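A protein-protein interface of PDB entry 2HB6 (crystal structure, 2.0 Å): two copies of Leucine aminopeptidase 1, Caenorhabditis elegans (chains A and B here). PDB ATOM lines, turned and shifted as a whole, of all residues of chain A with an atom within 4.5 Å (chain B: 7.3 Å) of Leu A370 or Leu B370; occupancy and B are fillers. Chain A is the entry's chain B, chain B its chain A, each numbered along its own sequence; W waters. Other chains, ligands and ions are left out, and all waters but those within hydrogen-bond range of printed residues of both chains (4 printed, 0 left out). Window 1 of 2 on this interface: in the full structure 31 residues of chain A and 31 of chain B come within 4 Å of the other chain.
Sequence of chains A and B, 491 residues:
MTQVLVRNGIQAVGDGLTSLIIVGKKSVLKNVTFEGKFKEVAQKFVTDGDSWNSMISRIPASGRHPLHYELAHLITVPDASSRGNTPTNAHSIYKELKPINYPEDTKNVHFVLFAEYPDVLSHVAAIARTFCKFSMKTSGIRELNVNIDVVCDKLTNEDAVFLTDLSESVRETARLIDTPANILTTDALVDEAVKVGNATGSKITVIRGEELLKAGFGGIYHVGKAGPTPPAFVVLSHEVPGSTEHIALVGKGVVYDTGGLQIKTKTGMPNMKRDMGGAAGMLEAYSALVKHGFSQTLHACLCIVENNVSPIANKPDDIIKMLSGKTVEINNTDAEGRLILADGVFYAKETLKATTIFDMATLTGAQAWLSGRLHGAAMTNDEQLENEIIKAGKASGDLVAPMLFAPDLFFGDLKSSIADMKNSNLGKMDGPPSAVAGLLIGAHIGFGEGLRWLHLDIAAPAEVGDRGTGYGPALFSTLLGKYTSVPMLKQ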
ATOM      1  N   ALA A 366      23.680 -24.007  17.397  1.00  0.00           N
ATOM      2  CA  ALA A 366      22.611 -23.084  17.713  1.00  0.00           C
ATOM      3  C   ALA A 366      21.259 -23.598  17.225  1.00  0.00           C
ATOM      4  O   ALA A 366      20.223 -23.188  17.749  1.00  0.00           O
ATOM      5  CB  ALA A 366      22.903 -21.728  17.121  1.00  0.00           C
ATOM      6  N   GLN A 367      21.255 -24.488  16.224  1.00  0.00           N
ATOM      7  CA  GLN A 367      19.989 -24.990  15.671  1.00  0.00           C
ATOM      8  C   GLN A 367      19.112 -25.647  16.745  1.00  0.00           C
ATOM      9  O   GLN A 367      17.893 -25.449  16.776  1.00  0.00           O
ATOM     10  CB  GLN A 367      20.237 -25.910  14.455  1.00  0.00           C
ATOM     11  CG  GLN A 367      19.019 -26.729  13.992  1.00  0.00           C
ATOM     12  CD  GLN A 367      18.852 -28.018  14.799  1.00  0.00           C
ATOM     13  OE1 GLN A 367      19.803 -28.788  14.969  1.00  0.00           O
ATOM     14  NE2 GLN A 367      17.663 -28.223  15.342  1.00  0.00           N
ATOM     15  N   ALA A 368      19.732 -26.424  17.637  1.00  0.00           N
ATOM     16  CA  ALA A 368      19.009 -27.050  18.748  1.00  0.00           C
ATOM     17  C   ALA A 368      18.325 -26.043  19.679  1.00  0.00           C
ATOM     18  O   ALA A 368      17.314 -26.364  20.306  1.00  0.00           O
ATOM     19  CB  ALA A 368      19.935 -27.966  19.541  1.00  0.00           C
ATOM     20  N   TRP A 369      18.858 -24.825  19.752  1.00  0.00           N
ATOM     21  CA  TRP A 369      18.254 -23.793  20.610  1.00  0.00           C
ATOM     22  C   TRP A 369      17.070 -23.105  19.920  1.00  0.00           C
ATOM     23  O   TRP A 369      16.279 -22.423  20.568  1.00  0.00           O
ATOM     24  CB  TRP A 369      19.299 -22.754  21.038  1.00  0.00           C
ATOM     25  CG  TRP A 369      20.392 -23.315  21.931  1.00  0.00           C
ATOM     26  CD1 TRP A 369      21.242 -24.353  21.641  1.00  0.00           C
ATOM     27  CD2 TRP A 369      20.758 -22.862  23.243  1.00  0.00           C
ATOM     28  NE1 TRP A 369      22.101 -24.575  22.691  1.00  0.00           N
ATOM     29  CE2 TRP A 369      21.826 -23.675  23.688  1.00  0.00           C
ATOM     30  CE3 TRP A 369      20.291 -21.851  24.085  1.00  0.00           C
ATOM     31  CZ2 TRP A 369      22.433 -23.500  24.935  1.00  0.00           C
ATOM     32  CZ3 TRP A 369      20.895 -21.684  25.335  1.00  0.00           C
ATOM     33  CH2 TRP A 369      21.950 -22.504  25.745  1.00  0.00           C
ATOM     34  N   LEU A 370      16.971 -23.267  18.606  1.00  0.00           N
ATOM     35  CA  LEU A 370      15.835 -22.741  17.839  1.00  0.00           C
ATOM     36  C   LEU A 370      14.699 -23.778  17.714  1.00  0.00           C
ATOM     37  O   LEU A 370      13.524 -23.484  17.987  1.00  0.00           O
ATOM     38  CB  LEU A 370      16.318 -22.296  16.459  1.00  0.00           C
ATOM     39  CG  LEU A 370      15.317 -21.482  15.634  1.00  0.00           C
ATOM     40  CD1 LEU A 370      16.074 -20.530  14.727  1.00  0.00           C
ATOM     41  CD2 LEU A 370      14.365 -22.384  14.826  1.00  0.00           C
ATOM     42  N   SER A 371      15.043 -24.990  17.278  1.00  0.00           N
ATOM     43  CA  SER A 371      14.008 -25.970  16.912  1.00  0.00           C
ATOM     44  C   SER A 371      14.110 -27.269  17.719  1.00  0.00           C
ATOM     45  O   SER A 371      13.342 -28.199  17.503  1.00  0.00           O
ATOM     46  CB  SER A 371      14.049 -26.256  15.397  1.00  0.00           C
ATOM     47  OG  SER A 371      15.254 -26.898  15.018  1.00  0.00           O
ATOM     48  N   GLY A 372      15.056 -27.339  18.650  1.00  0.00           N
ATOM     49  CA  GLY A 372      15.194 -28.552  19.470  1.00  0.00           C
ATOM     50  C   GLY A 372      15.937 -29.663  18.736  1.00  0.00           C
ATOM     51  O   GLY A 372      16.574 -29.419  17.712  1.00  0.00           O
ATOM     52  N   ALA A 377      15.617 -27.218  11.162  1.00  0.00           N
ATOM     53  CA  ALA A 377      15.214 -25.809  11.089  1.00  0.00           C
ATOM     54  C   ALA A 377      15.304 -25.306   9.654  1.00  0.00           C
ATOM     55  O   ALA A 377      16.388 -25.266   9.065  1.00  0.00           O
ATOM     56  CB  ALA A 377      16.074 -24.949  12.056  1.00  0.00           C
ATOM     57  N   PRO A 402       9.963 -24.019  11.365  1.00  0.00           N
ATOM     58  CA  PRO A 402      10.422 -22.864  10.591  1.00  0.00           C
ATOM     59  C   PRO A 402      11.381 -21.922  11.339  1.00  0.00           C
ATOM     60  O   PRO A 402      11.276 -21.771  12.564  1.00  0.00           O
ATOM     61  CB  PRO A 402       9.119 -22.129  10.247  1.00  0.00           C
ATOM     62  CG  PRO A 402       8.163 -22.490  11.329  1.00  0.00           C
ATOM     63  CD  PRO A 402       8.624 -23.808  11.961  1.00  0.00           C
ATOM     64  N   MET A 403      12.306 -21.333  10.579  1.00  0.00           N
ATOM     65  CA  MET A 403      13.175 -20.233  11.021  1.00  0.00           C
ATOM     66  C   MET A 403      12.615 -18.949  10.433  1.00  0.00           C
ATOM     67  O   MET A 403      12.123 -18.972   9.307  1.00  0.00           O
ATOM     68  CB  MET A 403      14.554 -20.395  10.377  1.00  0.00           C
ATOM     69  CG  MET A 403      15.584 -21.142  11.150  1.00  0.00           C
ATOM     70  SD  MET A 403      17.197 -20.724  10.461  1.00  0.00           S
ATOM     71  CE  MET A 403      17.783 -22.321   9.900  1.00  0.00           C
ATOM     72  N   PRO A 432      18.599 -14.903  14.905  1.00  0.00           N
ATOM     73  CA  PRO A 432      19.000 -16.201  15.482  1.00  0.00           C
ATOM     74  C   PRO A 432      20.274 -16.697  14.771  1.00  0.00           C
ATOM     75  O   PRO A 432      20.380 -16.570  13.556  1.00  0.00           O
ATOM     76  CB  PRO A 432      17.804 -17.128  15.189  1.00  0.00           C
ATOM     77  CG  PRO A 432      16.742 -16.292  14.518  1.00  0.00           C
ATOM     78  CD  PRO A 432      17.276 -14.924  14.233  1.00  0.00           C
ATOM     79  N   GLY B 365      18.053 -16.176  27.956  1.00  0.00           N
ATOM     80  CA  GLY B 365      18.978 -15.632  27.016  1.00  0.00           C
ATOM     81  C   GLY B 365      18.821 -16.516  25.788  1.00  0.00           C
ATOM     82  O   GLY B 365      19.130 -16.087  24.690  1.00  0.00           O
ATOM     83  N   ALA B 366      18.305 -17.739  25.975  1.00  0.00           N
ATOM     84  CA  ALA B 366      18.121 -18.646  24.860  1.00  0.00           C
ATOM     85  C   ALA B 366      17.111 -18.105  23.851  1.00  0.00           C
ATOM     86  O   ALA B 366      17.155 -18.488  22.672  1.00  0.00           O
ATOM     87  CB  ALA B 366      17.685 -20.002  25.354  1.00  0.00           C
ATOM     88  N   GLN B 367      16.205 -17.226  24.299  1.00  0.00           N
ATOM     89  CA  GLN B 367      15.172 -16.684  23.397  1.00  0.00           C
ATOM     90  C   GLN B 367      15.790 -16.031  22.151  1.00  0.00           C
ATOM     91  O   GLN B 367      15.311 -16.233  21.036  1.00  0.00           O
ATOM     92  CB  GLN B 367      14.195 -15.750  24.149  1.00  0.00           C
ATOM     93  CG  GLN B 367      13.259 -14.917  23.246  1.00  0.00           C
ATOM     94  CD  GLN B 367      13.938 -13.631  22.757  1.00  0.00           C
ATOM     95  OE1 GLN B 367      14.501 -12.872  23.552  1.00  0.00           O
ATOM     96  NE2 GLN B 367      13.927 -13.416  21.455  1.00  0.00           N
ATOM     97  N   ALA B 368      16.867 -15.263  22.337  1.00  0.00           N
ATOM     98  CA  ALA B 368      17.560 -14.631  21.201  1.00  0.00           C
ATOM     99  C   ALA B 368      18.128 -15.631  20.191  1.00  0.00           C
ATOM    100  O   ALA B 368      18.299 -15.299  19.016  1.00  0.00           O
ATOM    101  CB  ALA B 368      18.670 -13.688  21.693  1.00  0.00           C
ATOM    102  N   TRP B 369      18.416 -16.855  20.633  1.00  0.00           N
ATOM    103  CA  TRP B 369      18.897 -17.891  19.706  1.00  0.00           C
ATOM    104  C   TRP B 369      17.758 -18.547  18.919  1.00  0.00           C
ATOM    105  O   TRP B 369      17.993 -19.223  17.918  1.00  0.00           O
ATOM    106  CB  TRP B 369      19.715 -18.957  20.446  1.00  0.00           C
ATOM    107  CG  TRP B 369      20.997 -18.417  21.065  1.00  0.00           C
ATOM    108  CD1 TRP B 369      21.107 -17.390  21.971  1.00  0.00           C
ATOM    109  CD2 TRP B 369      22.333 -18.882  20.832  1.00  0.00           C
ATOM    110  NE1 TRP B 369      22.425 -17.189  22.308  1.00  0.00           N
ATOM    111  CE2 TRP B 369      23.198 -18.090  21.622  1.00  0.00           C
ATOM    112  CE3 TRP B 369      22.882 -19.889  20.041  1.00  0.00           C
ATOM    113  CZ2 TRP B 369      24.582 -18.283  21.640  1.00  0.00           C
ATOM    114  CZ3 TRP B 369      24.266 -20.076  20.055  1.00  0.00           C
ATOM    115  CH2 TRP B 369      25.096 -19.275  20.848  1.00  0.00           C
ATOM    116  N   LEU B 370      16.528 -18.365  19.388  1.00  0.00           N
ATOM    117  CA  LEU B 370      15.345 -18.871  18.692  1.00  0.00           C
ATOM    118  C   LEU B 370      14.752 -17.828  17.718  1.00  0.00           C
ATOM    119  O   LEU B 370      14.492 -18.121  16.546  1.00  0.00           O
ATOM    120  CB  LEU B 370      14.302 -19.327  19.720  1.00  0.00           C
ATOM    121  CG  LEU B 370      13.119 -20.123  19.154  1.00  0.00           C
ATOM    122  CD1 LEU B 370      12.584 -21.075  20.204  1.00  0.00           C
ATOM    123  CD2 LEU B 370      12.006 -19.192  18.636  1.00  0.00           C
ATOM    124  N   SER B 371      14.522 -16.613  18.211  1.00  0.00           N
ATOM    125  CA  SER B 371      13.778 -15.621  17.436  1.00  0.00           C
ATOM    126  C   SER B 371      14.573 -14.332  17.195  1.00  0.00           C
ATOM    127  O   SER B 371      14.054 -13.380  16.615  1.00  0.00           O
ATOM    128  CB  SER B 371      12.424 -15.308  18.112  1.00  0.00           C
ATOM    129  OG  SER B 371      12.602 -14.721  19.393  1.00  0.00           O
ATOM    130  N   GLY B 372      15.824 -14.293  17.645  1.00  0.00           N
ATOM    131  CA  GLY B 372      16.637 -13.085  17.465  1.00  0.00           C
ATOM    132  C   GLY B 372      16.296 -11.977  18.460  1.00  0.00           C
ATOM    133  O   GLY B 372      15.651 -12.224  19.483  1.00  0.00           O
ATOM    134  N   HIS B 375      12.210  -9.972  17.703  1.00  0.00           N
ATOM    135  CA  HIS B 375      10.967 -10.740  17.802  1.00  0.00           C
ATOM    136  C   HIS B 375      10.855 -11.360  19.185  1.00  0.00           C
ATOM    137  O   HIS B 375      11.758 -12.070  19.631  1.00  0.00           O
ATOM    138  CB  HIS B 375      10.924 -11.896  16.758  1.00  0.00           C
ATOM    139  CG  HIS B 375      10.871 -11.443  15.338  1.00  0.00           C
ATOM    140  ND1 HIS B 375      11.927 -10.815  14.716  1.00  0.00           N
ATOM    141  CD2 HIS B 375       9.897 -11.567  14.395  1.00  0.00           C
ATOM    142  CE1 HIS B 375      11.610 -10.560  13.459  1.00  0.00           C
ATOM    143  NE2 HIS B 375      10.379 -10.992  13.242  1.00  0.00           N
ATOM    144  N   GLY B 376       9.736 -11.118  19.853  1.00  0.00           N
ATOM    145  CA  GLY B 376       9.315 -11.960  20.953  1.00  0.00           C
ATOM    146  C   GLY B 376       9.067 -13.375  20.457  1.00  0.00           C
ATOM    147  O   GLY B 376       8.690 -13.578  19.304  1.00  0.00           O
ATOM    148  N   ALA B 377       9.280 -14.355  21.330  1.00  0.00           N
ATOM    149  CA  ALA B 377       9.012 -15.752  20.995  1.00  0.00           C
ATOM    150  C   ALA B 377       7.739 -16.242  21.683  1.00  0.00           C
ATOM    151  O   ALA B 377       7.664 -16.293  22.915  1.00  0.00           O
ATOM    152  CB  ALA B 377      10.234 -16.639  21.372  1.00  0.00           C
ATOM    153  N   ALA B 378       6.740 -16.593  20.867  1.00  0.00           N
ATOM    154  CA  ALA B 378       5.413 -16.974  21.332  1.00  0.00           C
ATOM    155  C   ALA B 378       5.209 -18.482  21.221  1.00  0.00           C
ATOM    156  O   ALA B 378       5.386 -19.068  20.146  1.00  0.00           O
ATOM    157  CB  ALA B 378       4.328 -16.263  20.500  1.00  0.00           C
ATOM    158  N   ALA B 401       7.591 -13.970  16.801  1.00  0.00           N
ATOM    159  CA  ALA B 401       7.891 -15.175  16.020  1.00  0.00           C
ATOM    160  C   ALA B 401       7.408 -16.388  16.816  1.00  0.00           C
ATOM    161  O   ALA B 401       7.353 -16.344  18.049  1.00  0.00           O
ATOM    162  CB  ALA B 401       9.412 -15.251  15.753  1.00  0.00           C
ATOM    163  N   PRO B 402       7.009 -17.466  16.123  1.00  0.00           N
ATOM    164  CA  PRO B 402       6.490 -18.614  16.863  1.00  0.00           C
ATOM    165  C   PRO B 402       7.562 -19.585  17.395  1.00  0.00           C
ATOM    166  O   PRO B 402       8.616 -19.744  16.783  1.00  0.00           O
ATOM    167  CB  PRO B 402       5.590 -19.319  15.837  1.00  0.00           C
ATOM    168  CG  PRO B 402       6.186 -18.975  14.500  1.00  0.00           C
ATOM    169  CD  PRO B 402       6.953 -17.659  14.656  1.00  0.00           C
ATOM    170  N   MET B 403       7.257 -20.188  18.542  1.00  0.00           N
ATOM    171  CA  MET B 403       8.016 -21.293  19.139  1.00  0.00           C
ATOM    172  C   MET B 403       7.221 -22.563  18.898  1.00  0.00           C
ATOM    173  O   MET B 403       5.993 -22.525  18.983  1.00  0.00           O
ATOM    174  CB  MET B 403       8.017 -21.125  20.659  1.00  0.00           C
ATOM    175  CG  MET B 403       9.172 -20.417  21.255  1.00  0.00           C
ATOM    176  SD  MET B 403       9.234 -20.852  22.997  1.00  0.00           S
ATOM    177  CE  MET B 403       8.997 -19.256  23.774  1.00  0.00           C
ATOM    178  N   LEU B 404       7.902 -23.684  18.661  1.00  0.00           N
ATOM    179  CA  LEU B 404       7.236 -24.997  18.724  1.00  0.00           C
ATOM    180  C   LEU B 404       6.434 -25.236  19.992  1.00  0.00           C
ATOM    181  O   LEU B 404       6.911 -24.986  21.114  1.00  0.00           O
ATOM    182  CB  LEU B 404       8.250 -26.146  18.561  1.00  0.00           C
ATOM    183  CG  LEU B 404       8.824 -26.382  17.174  1.00  0.00           C
ATOM    184  CD1 LEU B 404      10.018 -27.350  17.286  1.00  0.00           C
ATOM    185  CD2 LEU B 404       7.756 -26.907  16.174  1.00  0.00           C
ATOM    186  N   GLY B 431      14.001 -30.159  23.692  1.00  0.00           N
ATOM    187  CA  GLY B 431      13.282 -28.951  23.247  1.00  0.00           C
ATOM    188  C   GLY B 431      14.193 -27.744  23.100  1.00  0.00           C
ATOM    189  O   GLY B 431      15.276 -27.707  23.679  1.00  0.00           O
ATOM    190  N   PRO B 432      13.745 -26.728  22.352  1.00  0.00           N
ATOM    191  CA  PRO B 432      14.458 -25.445  22.476  1.00  0.00           C
ATOM    192  C   PRO B 432      14.357 -24.963  23.936  1.00  0.00           C
ATOM    193  O   PRO B 432      13.288 -25.078  24.536  1.00  0.00           O
ATOM    194  CB  PRO B 432      13.697 -24.503  21.530  1.00  0.00           C
ATOM    195  CG  PRO B 432      12.633 -25.305  20.863  1.00  0.00           C
ATOM    196  CD  PRO B 432      12.591 -26.686  21.429  1.00  0.00           C
ATOM    197  N   PRO B 433      15.476 -24.529  24.547  1.00  0.00           N
ATOM    198  CA  PRO B 433      15.381 -24.120  25.963  1.00  0.00           C
ATOM    199  C   PRO B 433      14.286 -23.100  26.308  1.00  0.00           C
ATOM    200  O   PRO B 433      13.659 -23.220  27.369  1.00  0.00           O
ATOM    201  CB  PRO B 433      16.780 -23.555  26.256  1.00  0.00           C
ATOM    202  CG  PRO B 433      17.692 -24.393  25.348  1.00  0.00           C
ATOM    203  CD  PRO B 433      16.867 -24.450  24.054  1.00  0.00           C
ATOM    204  N   SER B 434      14.041 -22.133  25.423  1.00  0.00           N
ATOM    205  CA  SER B 434      12.962 -21.150  25.622  1.00  0.00           C
ATOM    206  C   SER B 434      11.582 -21.777  25.629  1.00  0.00           C
ATOM    207  O   SER B 434      10.705 -21.337  26.383  1.00  0.00           O
ATOM    208  CB  SER B 434      13.018 -20.061  24.557  1.00  0.00           C
ATOM    209  OG  SER B 434      14.288 -19.442  24.590  1.00  0.00           O
ATOM    210  N   ALA B 435      11.392 -22.796  24.794  1.00  0.00           N
ATOM    211  CA  ALA B 435      10.167 -23.600  24.828  1.00  0.00           C
ATOM    212  C   ALA B 435      10.021 -24.380  26.123  1.00  0.00           C
ATOM    213  O   ALA B 435       8.942 -24.395  26.736  1.00  0.00           O
ATOM    214  CB  ALA B 435      10.096 -24.541  23.624  1.00  0.00           C
HETATM  215  O   HOH W   1      19.883 -20.208  16.284  1.00  0.00           O
HETATM  216  O   HOH W   2      15.579 -21.451  22.968  1.00  0.00           O
HETATM  217  O   HOH W   3      10.721 -23.242  17.779  1.00  0.00           O
HETATM  218  O   HOH W   4      17.735 -28.116  22.700  1.00  0.00           O
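Printed residues of chain B within 4 Å of Ala A368: Pro B432 (3.7 Å). Of the printed residues of chain B, Trp A369 touches Ala B366, Trp B369, Leu B370, Pro B432 and Pro B433. Leu A370 touches three residues of chain B. Leu B370 touches three residues of chain A. His B375 touches none of the printed residues of chain A. Of the printed residues of chain A, Gly B431 touches Gly A372 (3.9 Å). Of the printed residues of chain A, Pro B433 touches Trp A369 (3.8 Å). Ala B435 touches none of the printed residues of chain A. The nearest printed residue of chain A that does not touch Pro B432 is Gln A367 (6.4 Å).
Water W4 lies within hydrogen-bond range of the backbone carbonyl oxygen (O) of Gly B431 (2.7 Å) and the backbone carbonyl oxygen (O) of Ala A368 (3.0 Å). Water W2 lies within hydrogen-bond range of O of Trp A369 (2.7 Å), OG of Ser B434 (2.9 Å) and O of Ala B366 (3.4 Å). Water W1 lies within hydrogen-bond range of O of Trp B369 (2.7 Å) and O of Ala A366 (3.3 Å). Water W3 lies within hydrogen-bond range of O of Leu A370 (2.8 Å) and N of Leu B404 (3.0 Å).
Leu B370 touches Trp A369 (CB to O, 3.8 Å). Trp A369 touches Pro B432. Trp A369 touches Pro B433 (CA to CD, 3.8 Å). CB of Leu A370 touches O of Trp B369 (3.8 Å). CG of Pro B432 touches O of Leu A370, 3.5 Å away. Leu B404 touches Ser A371. Ala B368 touches Pro A432. Pro A432 touches Trp B369 (CB to O, 3.4 Å). Pro A432 touches Leu B370. C of Ser B371 touches CG of Pro A432 (3.96 Å).
The side-chain hydroxyl (OG) of Ser B371 lies within hydrogen-bond range of the backbone carbonyl oxygen (O) of His B375 (2.8 Å). The backbone carbonyl oxygen (O) of Gly A372 lies within hydrogen-bond range of the side-chain amide nitrogen (NE2) of Gln A367 (2.9 Å). OG of Ser B371 lies within hydrogen-bond range of NE2 of Gln B367 (2.8 Å). The side-chain hydroxyl (OG) of Ser A371 sits at hydrogen-bond distance from the side-chain amide nitrogen (NE2) of Gln A367, 2.8 Å away. NE2 of Gln B367 is in hydrogen-bond range of O of Gly B372 (2.9 Å).
Ala A368 touches Pro B432, and with the chains exchanged Pro A432 touches Ala B368. Leu A370 touches Pro B432, and with the chains exchanged Pro A432 touches Leu B370. Ser A371 touches Pro B432, and with the chains exchanged Pro A432 touches Ser B371. Gly A372 touches Pro B432, and with the chains exchanged Pro A432 touches Gly B372. 11 positions are printed for both chains. Of the 19 pairs that touch across the chains among the printed residues, 16 have their exchanged pair printed and touching as well.
Of the 21 printed residues of chain B, 10 touch a printed residue of chain A. Printed residues of chain B that touch a printed residue of chain A: Ala B366, Ala B368, Trp B369, Leu B370, Ser B371, Gly B372, Leu B404, Gly B431, Pro B432 and Pro B433. Hydrophobic or aromatic side chains of chain B that line the printed part of chain A: Ala B366, Trp B369, Leu B370, Leu B404, Pro B432 and Pro B433. Hydrophobic or aromatic side chains of chain A that line the printed part of chain B: Ala A366, Trp A369, Leu A370 and Pro A432. Among the printed residues, 19 pairs touch across the chains.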
